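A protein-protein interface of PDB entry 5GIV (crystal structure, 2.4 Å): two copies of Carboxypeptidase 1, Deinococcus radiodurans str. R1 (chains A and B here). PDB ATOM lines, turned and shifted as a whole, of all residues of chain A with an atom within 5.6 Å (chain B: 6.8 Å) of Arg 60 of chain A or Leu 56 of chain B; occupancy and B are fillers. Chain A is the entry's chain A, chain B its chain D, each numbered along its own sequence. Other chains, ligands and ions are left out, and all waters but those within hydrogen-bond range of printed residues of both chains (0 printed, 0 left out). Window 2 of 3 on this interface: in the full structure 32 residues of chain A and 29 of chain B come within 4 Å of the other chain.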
ATOM      1  N   HIS A  16      27.980   2.798  -9.091  1.00  0.00           N
ATOM      2  CA  HIS A  16      27.143   3.707  -8.319  1.00  0.00           C
ATOM      3  C   HIS A  16      27.381   5.147  -8.736  1.00  0.00           C
ATOM      4  O   HIS A  16      26.435   5.940  -8.820  1.00  0.00           O
ATOM      5  CB  HIS A  16      27.408   3.521  -6.827  1.00  0.00           C
ATOM      6  CG  HIS A  16      26.354   4.114  -5.945  1.00  0.00           C
ATOM      7  ND1 HIS A  16      25.195   3.442  -5.613  1.00  0.00           N
ATOM      8  CD2 HIS A  16      26.297   5.302  -5.298  1.00  0.00           C
ATOM      9  CE1 HIS A  16      24.462   4.200  -4.816  1.00  0.00           C
ATOM     10  NE2 HIS A  16      25.113   5.329  -4.600  1.00  0.00           N
ATOM     11  N   GLU A  19      25.597   5.696 -11.868  1.00  0.00           N
ATOM     12  CA  GLU A  19      24.167   5.788 -11.599  1.00  0.00           C
ATOM     13  C   GLU A  19      23.810   7.174 -11.075  1.00  0.00           C
ATOM     14  O   GLU A  19      22.757   7.725 -11.420  1.00  0.00           O
ATOM     15  CB  GLU A  19      23.748   4.686 -10.616  1.00  0.00           C
ATOM     16  CG  GLU A  19      22.230   4.551 -10.417  1.00  0.00           C
ATOM     17  CD  GLU A  19      21.836   3.382  -9.520  1.00  0.00           C
ATOM     18  OE1 GLU A  19      20.817   3.495  -8.801  1.00  0.00           O
ATOM     19  OE2 GLU A  19      22.537   2.347  -9.528  1.00  0.00           O
ATOM     20  N   LEU A  20      24.679   7.756 -10.239  1.00  0.00           N
ATOM     21  CA  LEU A  20      24.454   9.126  -9.785  1.00  0.00           C
ATOM     22  C   LEU A  20      24.495  10.105 -10.948  1.00  0.00           C
ATOM     23  O   LEU A  20      23.659  11.010 -11.036  1.00  0.00           O
ATOM     24  CB  LEU A  20      25.479   9.516  -8.719  1.00  0.00           C
ATOM     25  CG  LEU A  20      25.343   8.768  -7.386  1.00  0.00           C
ATOM     26  CD1 LEU A  20      26.422   9.186  -6.396  1.00  0.00           C
ATOM     27  CD2 LEU A  20      23.950   8.981  -6.791  1.00  0.00           C
ATOM     28  N   PHE A  23      21.173   9.628 -13.046  1.00  0.00           N
ATOM     29  CA  PHE A  23      20.079  10.380 -12.445  1.00  0.00           C
ATOM     30  C   PHE A  23      20.225  11.862 -12.751  1.00  0.00           C
ATOM     31  O   PHE A  23      19.254  12.529 -13.123  1.00  0.00           O
ATOM     32  CB  PHE A  23      20.036  10.169 -10.930  1.00  0.00           C
ATOM     33  CG  PHE A  23      19.243   8.970 -10.499  1.00  0.00           C
ATOM     34  CD1 PHE A  23      17.854   8.992 -10.533  1.00  0.00           C
ATOM     35  CD2 PHE A  23      19.878   7.839 -10.010  1.00  0.00           C
ATOM     36  CE1 PHE A  23      17.114   7.891 -10.128  1.00  0.00           C
ATOM     37  CE2 PHE A  23      19.143   6.729  -9.597  1.00  0.00           C
ATOM     38  CZ  PHE A  23      17.758   6.759  -9.654  1.00  0.00           C
ATOM     39  N   LEU A  53      12.041  12.105  -9.077  1.00  0.00           N
ATOM     40  CA  LEU A  53      13.431  11.804  -9.400  1.00  0.00           C
ATOM     41  C   LEU A  53      14.385  12.410  -8.380  1.00  0.00           C
ATOM     42  O   LEU A  53      15.397  11.792  -8.027  1.00  0.00           O
ATOM     43  CB  LEU A  53      13.775  12.298 -10.800  1.00  0.00           C
ATOM     44  CG  LEU A  53      13.752  11.255 -11.916  1.00  0.00           C
ATOM     45  CD1 LEU A  53      14.531  11.791 -13.116  1.00  0.00           C
ATOM     46  CD2 LEU A  53      14.304   9.903 -11.449  1.00  0.00           C
ATOM     47  N   GLY A  55      13.849  12.658  -5.255  1.00  0.00           N
ATOM     48  CA  GLY A  55      13.844  11.748  -4.119  1.00  0.00           C
ATOM     49  C   GLY A  55      14.688  10.510  -4.348  1.00  0.00           C
ATOM     50  O   GLY A  55      15.449  10.096  -3.470  1.00  0.00           O
ATOM     51  N   LEU A  56      14.566   9.895  -5.527  1.00  0.00           N
ATOM     52  CA  LEU A  56      15.355   8.699  -5.813  1.00  0.00           C
ATOM     53  C   LEU A  56      16.845   9.018  -5.832  1.00  0.00           C
ATOM     54  O   LEU A  56      17.656   8.299  -5.237  1.00  0.00           O
ATOM     55  CB  LEU A  56      14.923   8.076  -7.141  1.00  0.00           C
ATOM     56  CG  LEU A  56      13.531   7.445  -7.150  1.00  0.00           C
ATOM     57  CD1 LEU A  56      13.105   7.083  -8.558  1.00  0.00           C
ATOM     58  CD2 LEU A  56      13.506   6.219  -6.246  1.00  0.00           C
ATOM     59  N   ARG A  57      17.225  10.095  -6.516  1.00  0.00           N
ATOM     60  CA  ARG A  57      18.636  10.449  -6.594  1.00  0.00           C
ATOM     61  C   ARG A  57      19.201  10.774  -5.217  1.00  0.00           C
ATOM     62  O   ARG A  57      20.312  10.355  -4.877  1.00  0.00           O
ATOM     63  CB  ARG A  57      18.822  11.622  -7.556  1.00  0.00           C
ATOM     64  CG  ARG A  57      20.201  12.220  -7.542  1.00  0.00           C
ATOM     65  CD  ARG A  57      20.245  13.435  -6.634  1.00  0.00           C
ATOM     66  NE  ARG A  57      19.316  14.478  -7.066  1.00  0.00           N
ATOM     67  CZ  ARG A  57      18.772  15.388  -6.257  1.00  0.00           C
ATOM     68  NH1 ARG A  57      19.057  15.381  -4.957  1.00  0.00           N
ATOM     69  NH2 ARG A  57      17.936  16.303  -6.744  1.00  0.00           N
ATOM     70  N   HIS A  58      18.433  11.492  -4.396  1.00  0.00           N
ATOM     71  CA  HIS A  58      18.909  11.820  -3.057  1.00  0.00           C
ATOM     72  C   HIS A  58      19.167  10.558  -2.249  1.00  0.00           C
ATOM     73  O   HIS A  58      20.177  10.456  -1.542  1.00  0.00           O
ATOM     74  CB  HIS A  58      17.889  12.707  -2.344  1.00  0.00           C
ATOM     75  CG  HIS A  58      18.285  13.079  -0.951  1.00  0.00           C
ATOM     76  ND1 HIS A  58      19.156  14.109  -0.672  1.00  0.00           N
ATOM     77  CD2 HIS A  58      17.946  12.541   0.245  1.00  0.00           C
ATOM     78  CE1 HIS A  58      19.316  14.209   0.636  1.00  0.00           C
ATOM     79  NE2 HIS A  58      18.595  13.265   1.213  1.00  0.00           N
ATOM     80  N   ALA A  59      18.278   9.572  -2.362  1.00  0.00           N
ATOM     81  CA  ALA A  59      18.489   8.303  -1.674  1.00  0.00           C
ATOM     82  C   ALA A  59      19.781   7.637  -2.140  1.00  0.00           C
ATOM     83  O   ALA A  59      20.599   7.200  -1.323  1.00  0.00           O
ATOM     84  CB  ALA A  59      17.290   7.383  -1.901  1.00  0.00           C
ATOM     85  N   ARG A  60      19.981   7.549  -3.456  1.00  0.00           N
ATOM     86  CA  ARG A  60      21.227   6.982  -3.960  1.00  0.00           C
ATOM     87  C   ARG A  60      22.427   7.725  -3.393  1.00  0.00           C
ATOM     88  O   ARG A  60      23.392   7.104  -2.935  1.00  0.00           O
ATOM     89  CB  ARG A  60      21.248   7.020  -5.486  1.00  0.00           C
ATOM     90  CG  ARG A  60      19.923   6.674  -6.133  1.00  0.00           C
ATOM     91  CD  ARG A  60      19.651   5.182  -6.152  1.00  0.00           C
ATOM     92  NE  ARG A  60      18.212   4.913  -6.072  1.00  0.00           N
ATOM     93  CZ  ARG A  60      17.601   3.879  -6.647  1.00  0.00           C
ATOM     94  NH1 ARG A  60      16.291   3.726  -6.503  1.00  0.00           N
ATOM     95  NH2 ARG A  60      18.294   3.008  -7.377  1.00  0.00           N
ATOM     96  N   ALA A  61      22.376   9.059  -3.395  1.00  0.00           N
ATOM     97  CA  ALA A  61      23.521   9.848  -2.955  1.00  0.00           C
ATOM     98  C   ALA A  61      23.818   9.667  -1.473  1.00  0.00           C
ATOM     99  O   ALA A  61      24.949   9.913  -1.046  1.00  0.00           O
ATOM    100  CB  ALA A  61      23.298  11.327  -3.273  1.00  0.00           C
ATOM    101  N   THR A  62      22.839   9.233  -0.680  1.00  0.00           N
ATOM    102  CA  THR A  62      23.034   9.052   0.752  1.00  0.00           C
ATOM    103  C   THR A  62      22.953   7.592   1.176  1.00  0.00           C
ATOM    104  O   THR A  62      22.885   7.311   2.379  1.00  0.00           O
ATOM    105  CB  THR A  62      22.005   9.867   1.536  1.00  0.00           C
ATOM    106  OG1 THR A  62      20.692   9.427   1.180  1.00  0.00           O
ATOM    107  CG2 THR A  62      22.140  11.351   1.228  1.00  0.00           C
ATOM    108  N   ASP A  63      22.988   6.655   0.227  1.00  0.00           N
ATOM    109  CA  ASP A  63      22.841   5.251   0.578  1.00  0.00           C
ATOM    110  C   ASP A  63      23.960   4.832   1.520  1.00  0.00           C
ATOM    111  O   ASP A  63      25.140   5.075   1.251  1.00  0.00           O
ATOM    112  CB  ASP A  63      22.860   4.392  -0.680  1.00  0.00           C
ATOM    113  CG  ASP A  63      22.748   2.918  -0.373  1.00  0.00           C
ATOM    114  OD1 ASP A  63      21.610   2.434  -0.198  1.00  0.00           O
ATOM    115  OD2 ASP A  63      23.799   2.247  -0.275  1.00  0.00           O
ATOM    116  N   TYR A  66      26.553   2.550  -0.037  1.00  0.00           N
ATOM    117  CA  TYR A  66      27.475   3.359  -0.831  1.00  0.00           C
ATOM    118  C   TYR A  66      28.492   4.061   0.059  1.00  0.00           C
ATOM    119  O   TYR A  66      29.693   4.076  -0.244  1.00  0.00           O
ATOM    120  CB  TYR A  66      26.675   4.373  -1.654  1.00  0.00           C
ATOM    121  CG  TYR A  66      27.484   5.472  -2.325  1.00  0.00           C
ATOM    122  CD1 TYR A  66      28.586   5.185  -3.119  1.00  0.00           C
ATOM    123  CD2 TYR A  66      27.133   6.808  -2.157  1.00  0.00           C
ATOM    124  CE1 TYR A  66      29.301   6.192  -3.732  1.00  0.00           C
ATOM    125  CE2 TYR A  66      27.850   7.819  -2.763  1.00  0.00           C
ATOM    126  CZ  TYR A  66      28.930   7.510  -3.547  1.00  0.00           C
ATOM    127  OH  TYR A  66      29.642   8.525  -4.147  1.00  0.00           O
ATOM    128  N   GLU B  19       2.762   6.934  -9.107  1.00  0.00           N
ATOM    129  CA  GLU B  19       4.201   6.784  -9.272  1.00  0.00           C
ATOM    130  C   GLU B  19       4.538   5.952 -10.505  1.00  0.00           C
ATOM    131  O   GLU B  19       5.506   6.256 -11.211  1.00  0.00           O
ATOM    132  CB  GLU B  19       4.814   6.181  -8.006  1.00  0.00           C
ATOM    133  CG  GLU B  19       6.338   6.129  -8.019  1.00  0.00           C
ATOM    134  CD  GLU B  19       6.937   5.643  -6.704  1.00  0.00           C
ATOM    135  OE1 GLU B  19       6.358   5.926  -5.632  1.00  0.00           O
ATOM    136  OE2 GLU B  19       7.983   4.964  -6.744  1.00  0.00           O
ATOM    137  N   LEU B  20       3.769   4.888 -10.778  1.00  0.00           N
ATOM    138  CA  LEU B  20       4.004   4.115 -11.999  1.00  0.00           C
ATOM    139  C   LEU B  20       3.740   4.955 -13.243  1.00  0.00           C
ATOM    140  O   LEU B  20       4.516   4.909 -14.208  1.00  0.00           O
ATOM    141  CB  LEU B  20       3.150   2.848 -12.009  1.00  0.00           C
ATOM    142  CG  LEU B  20       3.504   1.811 -10.940  1.00  0.00           C
ATOM    143  CD1 LEU B  20       2.553   0.632 -10.996  1.00  0.00           C
ATOM    144  CD2 LEU B  20       4.944   1.343 -11.108  1.00  0.00           C
ATOM    145  N   PHE B  23       6.819   7.286 -13.615  1.00  0.00           N
ATOM    146  CA  PHE B  23       7.942   6.587 -14.232  1.00  0.00           C
ATOM    147  C   PHE B  23       7.731   6.445 -15.731  1.00  0.00           C
ATOM    148  O   PHE B  23       8.650   6.696 -16.523  1.00  0.00           O
ATOM    149  CB  PHE B  23       8.135   5.208 -13.591  1.00  0.00           C
ATOM    150  CG  PHE B  23       8.989   5.223 -12.354  1.00  0.00           C
ATOM    151  CD1 PHE B  23      10.367   5.349 -12.450  1.00  0.00           C
ATOM    152  CD2 PHE B  23       8.422   5.103 -11.098  1.00  0.00           C
ATOM    153  CE1 PHE B  23      11.170   5.362 -11.316  1.00  0.00           C
ATOM    154  CE2 PHE B  23       9.218   5.115  -9.952  1.00  0.00           C
ATOM    155  CZ  PHE B  23      10.600   5.249 -10.069  1.00  0.00           C
ATOM    156  N   SER B  51      17.730   2.291 -19.504  1.00  0.00           N
ATOM    157  CA  SER B  51      17.783   1.046 -18.742  1.00  0.00           C
ATOM    158  C   SER B  51      17.697   1.308 -17.246  1.00  0.00           C
ATOM    159  O   SER B  51      17.038   0.555 -16.518  1.00  0.00           O
ATOM    160  CB  SER B  51      19.057   0.265 -19.061  1.00  0.00           C
ATOM    161  OG  SER B  51      19.128  -0.030 -20.439  1.00  0.00           O
ATOM    162  N   LEU B  52      18.363   2.362 -16.765  1.00  0.00           N
ATOM    163  CA  LEU B  52      18.266   2.691 -15.349  1.00  0.00           C
ATOM    164  C   LEU B  52      16.812   2.912 -14.940  1.00  0.00           C
ATOM    165  O   LEU B  52      16.370   2.412 -13.899  1.00  0.00           O
ATOM    166  CB  LEU B  52      19.122   3.922 -15.029  1.00  0.00           C
ATOM    167  CG  LEU B  52      19.011   4.453 -13.596  1.00  0.00           C
ATOM    168  CD1 LEU B  52      19.489   3.405 -12.602  1.00  0.00           C
ATOM    169  CD2 LEU B  52      19.824   5.729 -13.428  1.00  0.00           C
ATOM    170  N   LEU B  53      16.056   3.663 -15.746  1.00  0.00           N
ATOM    171  CA  LEU B  53      14.657   3.904 -15.411  1.00  0.00           C
ATOM    172  C   LEU B  53      13.815   2.653 -15.605  1.00  0.00           C
ATOM    173  O   LEU B  53      12.907   2.384 -14.809  1.00  0.00           O
ATOM    174  CB  LEU B  53      14.088   5.052 -16.244  1.00  0.00           C
ATOM    175  CG  LEU B  53      13.971   6.388 -15.524  1.00  0.00           C
ATOM    176  CD1 LEU B  53      13.049   7.313 -16.283  1.00  0.00           C
ATOM    177  CD2 LEU B  53      13.448   6.161 -14.122  1.00  0.00           C
ATOM    178  N   ALA B  54      14.107   1.866 -16.647  1.00  0.00           N
ATOM    179  CA  ALA B  54      13.371   0.622 -16.843  1.00  0.00           C
ATOM    180  C   ALA B  54      13.494  -0.280 -15.623  1.00  0.00           C
ATOM    181  O   ALA B  54      12.497  -0.845 -15.155  1.00  0.00           O
ATOM    182  CB  ALA B  54      13.870  -0.098 -18.092  1.00  0.00           C
ATOM    183  N   GLY B  55      14.701  -0.384 -15.062  1.00  0.00           N
ATOM    184  CA  GLY B  55      14.885  -1.226 -13.893  1.00  0.00           C
ATOM    185  C   GLY B  55      14.101  -0.730 -12.697  1.00  0.00           C
ATOM    186  O   GLY B  55      13.449  -1.512 -12.005  1.00  0.00           O
ATOM    187  N   LEU B  56      14.139   0.580 -12.449  1.00  0.00           N
ATOM    188  CA  LEU B  56      13.419   1.141 -11.311  1.00  0.00           C
ATOM    189  C   LEU B  56      11.915   0.940 -11.454  1.00  0.00           C
ATOM    190  O   LEU B  56      11.244   0.474 -10.524  1.00  0.00           O
ATOM    191  CB  LEU B  56      13.746   2.627 -11.178  1.00  0.00           C
ATOM    192  CG  LEU B  56      15.166   2.993 -10.761  1.00  0.00           C
ATOM    193  CD1 LEU B  56      15.382   4.480 -10.946  1.00  0.00           C
ATOM    194  CD2 LEU B  56      15.394   2.596  -9.312  1.00  0.00           C
ATOM    195  N   ARG B  57      11.369   1.272 -12.626  1.00  0.00           N
ATOM    196  CA  ARG B  57       9.933   1.140 -12.833  1.00  0.00           C
ATOM    197  C   ARG B  57       9.493  -0.312 -12.692  1.00  0.00           C
ATOM    198  O   ARG B  57       8.447  -0.597 -12.098  1.00  0.00           O
ATOM    199  CB  ARG B  57       9.553   1.703 -14.203  1.00  0.00           C
ATOM    200  CG  ARG B  57       8.135   1.404 -14.642  1.00  0.00           C
ATOM    201  CD  ARG B  57       8.128   0.173 -15.526  1.00  0.00           C
ATOM    202  NE  ARG B  57       8.973   0.370 -16.700  1.00  0.00           N
ATOM    203  CZ  ARG B  57       9.582  -0.610 -17.364  1.00  0.00           C
ATOM    204  NH1 ARG B  57       9.451  -1.870 -16.963  1.00  0.00           N
ATOM    205  NH2 ARG B  57      10.332  -0.325 -18.423  1.00  0.00           N
ATOM    206  N   HIS B  58      10.286  -1.246 -13.217  1.00  0.00           N
ATOM    207  CA  HIS B  58       9.935  -2.653 -13.087  1.00  0.00           C
ATOM    208  C   HIS B  58       9.915  -3.076 -11.623  1.00  0.00           C
ATOM    209  O   HIS B  58       9.049  -3.854 -11.204  1.00  0.00           O
ATOM    210  CB  HIS B  58      10.901  -3.517 -13.899  1.00  0.00           C
ATOM    211  CG  HIS B  58      10.598  -4.980 -13.827  1.00  0.00           C
ATOM    212  ND1 HIS B  58       9.595  -5.567 -14.571  1.00  0.00           N
ATOM    213  CD2 HIS B  58      11.161  -5.977 -13.104  1.00  0.00           C
ATOM    214  CE1 HIS B  58       9.554  -6.861 -14.310  1.00  0.00           C
ATOM    215  NE2 HIS B  58      10.496  -7.137 -13.425  1.00  0.00           N
ATOM    216  N   ALA B  59      10.863  -2.573 -10.828  1.00  0.00           N
ATOM    217  CA  ALA B  59      10.869  -2.881  -9.402  1.00  0.00           C
ATOM    218  C   ALA B  59       9.584  -2.410  -8.727  1.00  0.00           C
ATOM    219  O   ALA B  59       9.025  -3.115  -7.877  1.00  0.00           O
ATOM    220  CB  ALA B  59      12.084  -2.244  -8.730  1.00  0.00           C
ATOM    221  N   ARG B  60       9.109  -1.212  -9.079  1.00  0.00           N
ATOM    222  CA  ARG B  60       7.889  -0.706  -8.464  1.00  0.00           C
ATOM    223  C   ARG B  60       6.661  -1.425  -9.009  1.00  0.00           C
ATOM    224  O   ARG B  60       5.706  -1.683  -8.265  1.00  0.00           O
ATOM    225  CB  ARG B  60       7.773   0.803  -8.684  1.00  0.00           C
ATOM    226  CG  ARG B  60       9.079   1.567  -8.539  1.00  0.00           C
ATOM    227  CD  ARG B  60       9.667   1.494  -7.139  1.00  0.00           C
ATOM    228  NE  ARG B  60       8.872   2.230  -6.157  1.00  0.00           N
ATOM    229  CZ  ARG B  60       8.329   1.691  -5.063  1.00  0.00           C
ATOM    230  NH1 ARG B  60       8.505   0.398  -4.790  1.00  0.00           N
ATOM    231  NH2 ARG B  60       7.619   2.446  -4.228  1.00  0.00           N
ATOM    232  N   ALA B  61       6.663  -1.757 -10.304  1.00  0.00           N
ATOM    233  CA  ALA B  61       5.536  -2.480 -10.886  1.00  0.00           C
ATOM    234  C   ALA B  61       5.400  -3.881 -10.307  1.00  0.00           C
ATOM    235  O   ALA B  61       4.307  -4.459 -10.354  1.00  0.00           O
ATOM    236  CB  ALA B  61       5.677  -2.556 -12.408  1.00  0.00           C
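The side-chain carboxylate (OE1) of Glu 19 of chain A is in salt-bridge range of the guanidinium group (NH2) of Arg 60 of chain A.
A ring nitrogen (NE2) of His 16 of chain A sits at hydrogen-bond distance from the backbone carbonyl oxygen (O) of Arg 60 of chain A (3.0 Å).
Of the 15 printed residues of chain A, 4 touch a printed residue of chain B.
Hydrophobic or aromatic side chains of chain A that line the printed part of chain B: Phe 23 and Leu 56.
Of the 14 printed residues of chain B, 3 touch a printed residue of chain A.
Hydrophobic or aromatic side chains of chain B within 4 Å of the printed part of chain A: Phe 23, Leu 52 and Leu 56.
Along chain B the printed residues that touch a printed residue of chain A span positions 23 to 56.
Among the printed residues, 4 pairs touch across the chains.
Of the printed residues of chain B, Glu 19 of chain A touches Leu 52 (3.7 Å).
Of the printed residues of chain B, Phe 23 of chain A touches Leu 56 (3.5 Å).
Printed residues of chain B within 4 Å of Leu 56 of chain A: Phe 23 (3.5 Å).
Of chain B, only Leu 56 (3.2 Å) comes within 4 Å of Arg 60 of chain A.
Leu 20 of chain B touches none of the printed residues of chain A.
Printed residues of chain A within 4 Å of Phe 23 of chain B: Leu 56 (3.5 Å).
Leu 56 of chain B touches just these residues of chain A: Phe 23 (3.5 Å) and Arg 60 (3.2 Å).
Ala 61 of chain B touches none of the printed residues of chain A.
The nearest residue of chain A that does not touch Leu 56 of chain B is Leu 56 of chain A (4.2 Å).
Phe 23 of chain A touches Leu 56 of chain B, and with the chains exchanged Leu 56 of chain A touches Phe 23 of chain B.
Arg 60 of chain A touches Leu 56 of chain B, but with the chains exchanged Leu 56 of chain A does not touch Arg 60 of chain B (6.1 Å).
11 positions are printed for both chains.
Of the 4 pairs that touch across the chains among the printed residues, 2 have their exchanged pair printed and touching as well.
CD1 of Leu 52 of chain B touches CG of Glu 19 of chain A, 3.7 Å away.
Leu 56 of chain B touches Phe 23 of chain A (CD1 to CZ, 3.5 Å).
CD1 of Leu 56 of chain A touches CZ of Phe 23 of chain B, at 3.5 Å.
Arg 60 of chain A touches Leu 56 of chain B (NH1 to CD2, 3.2 Å).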
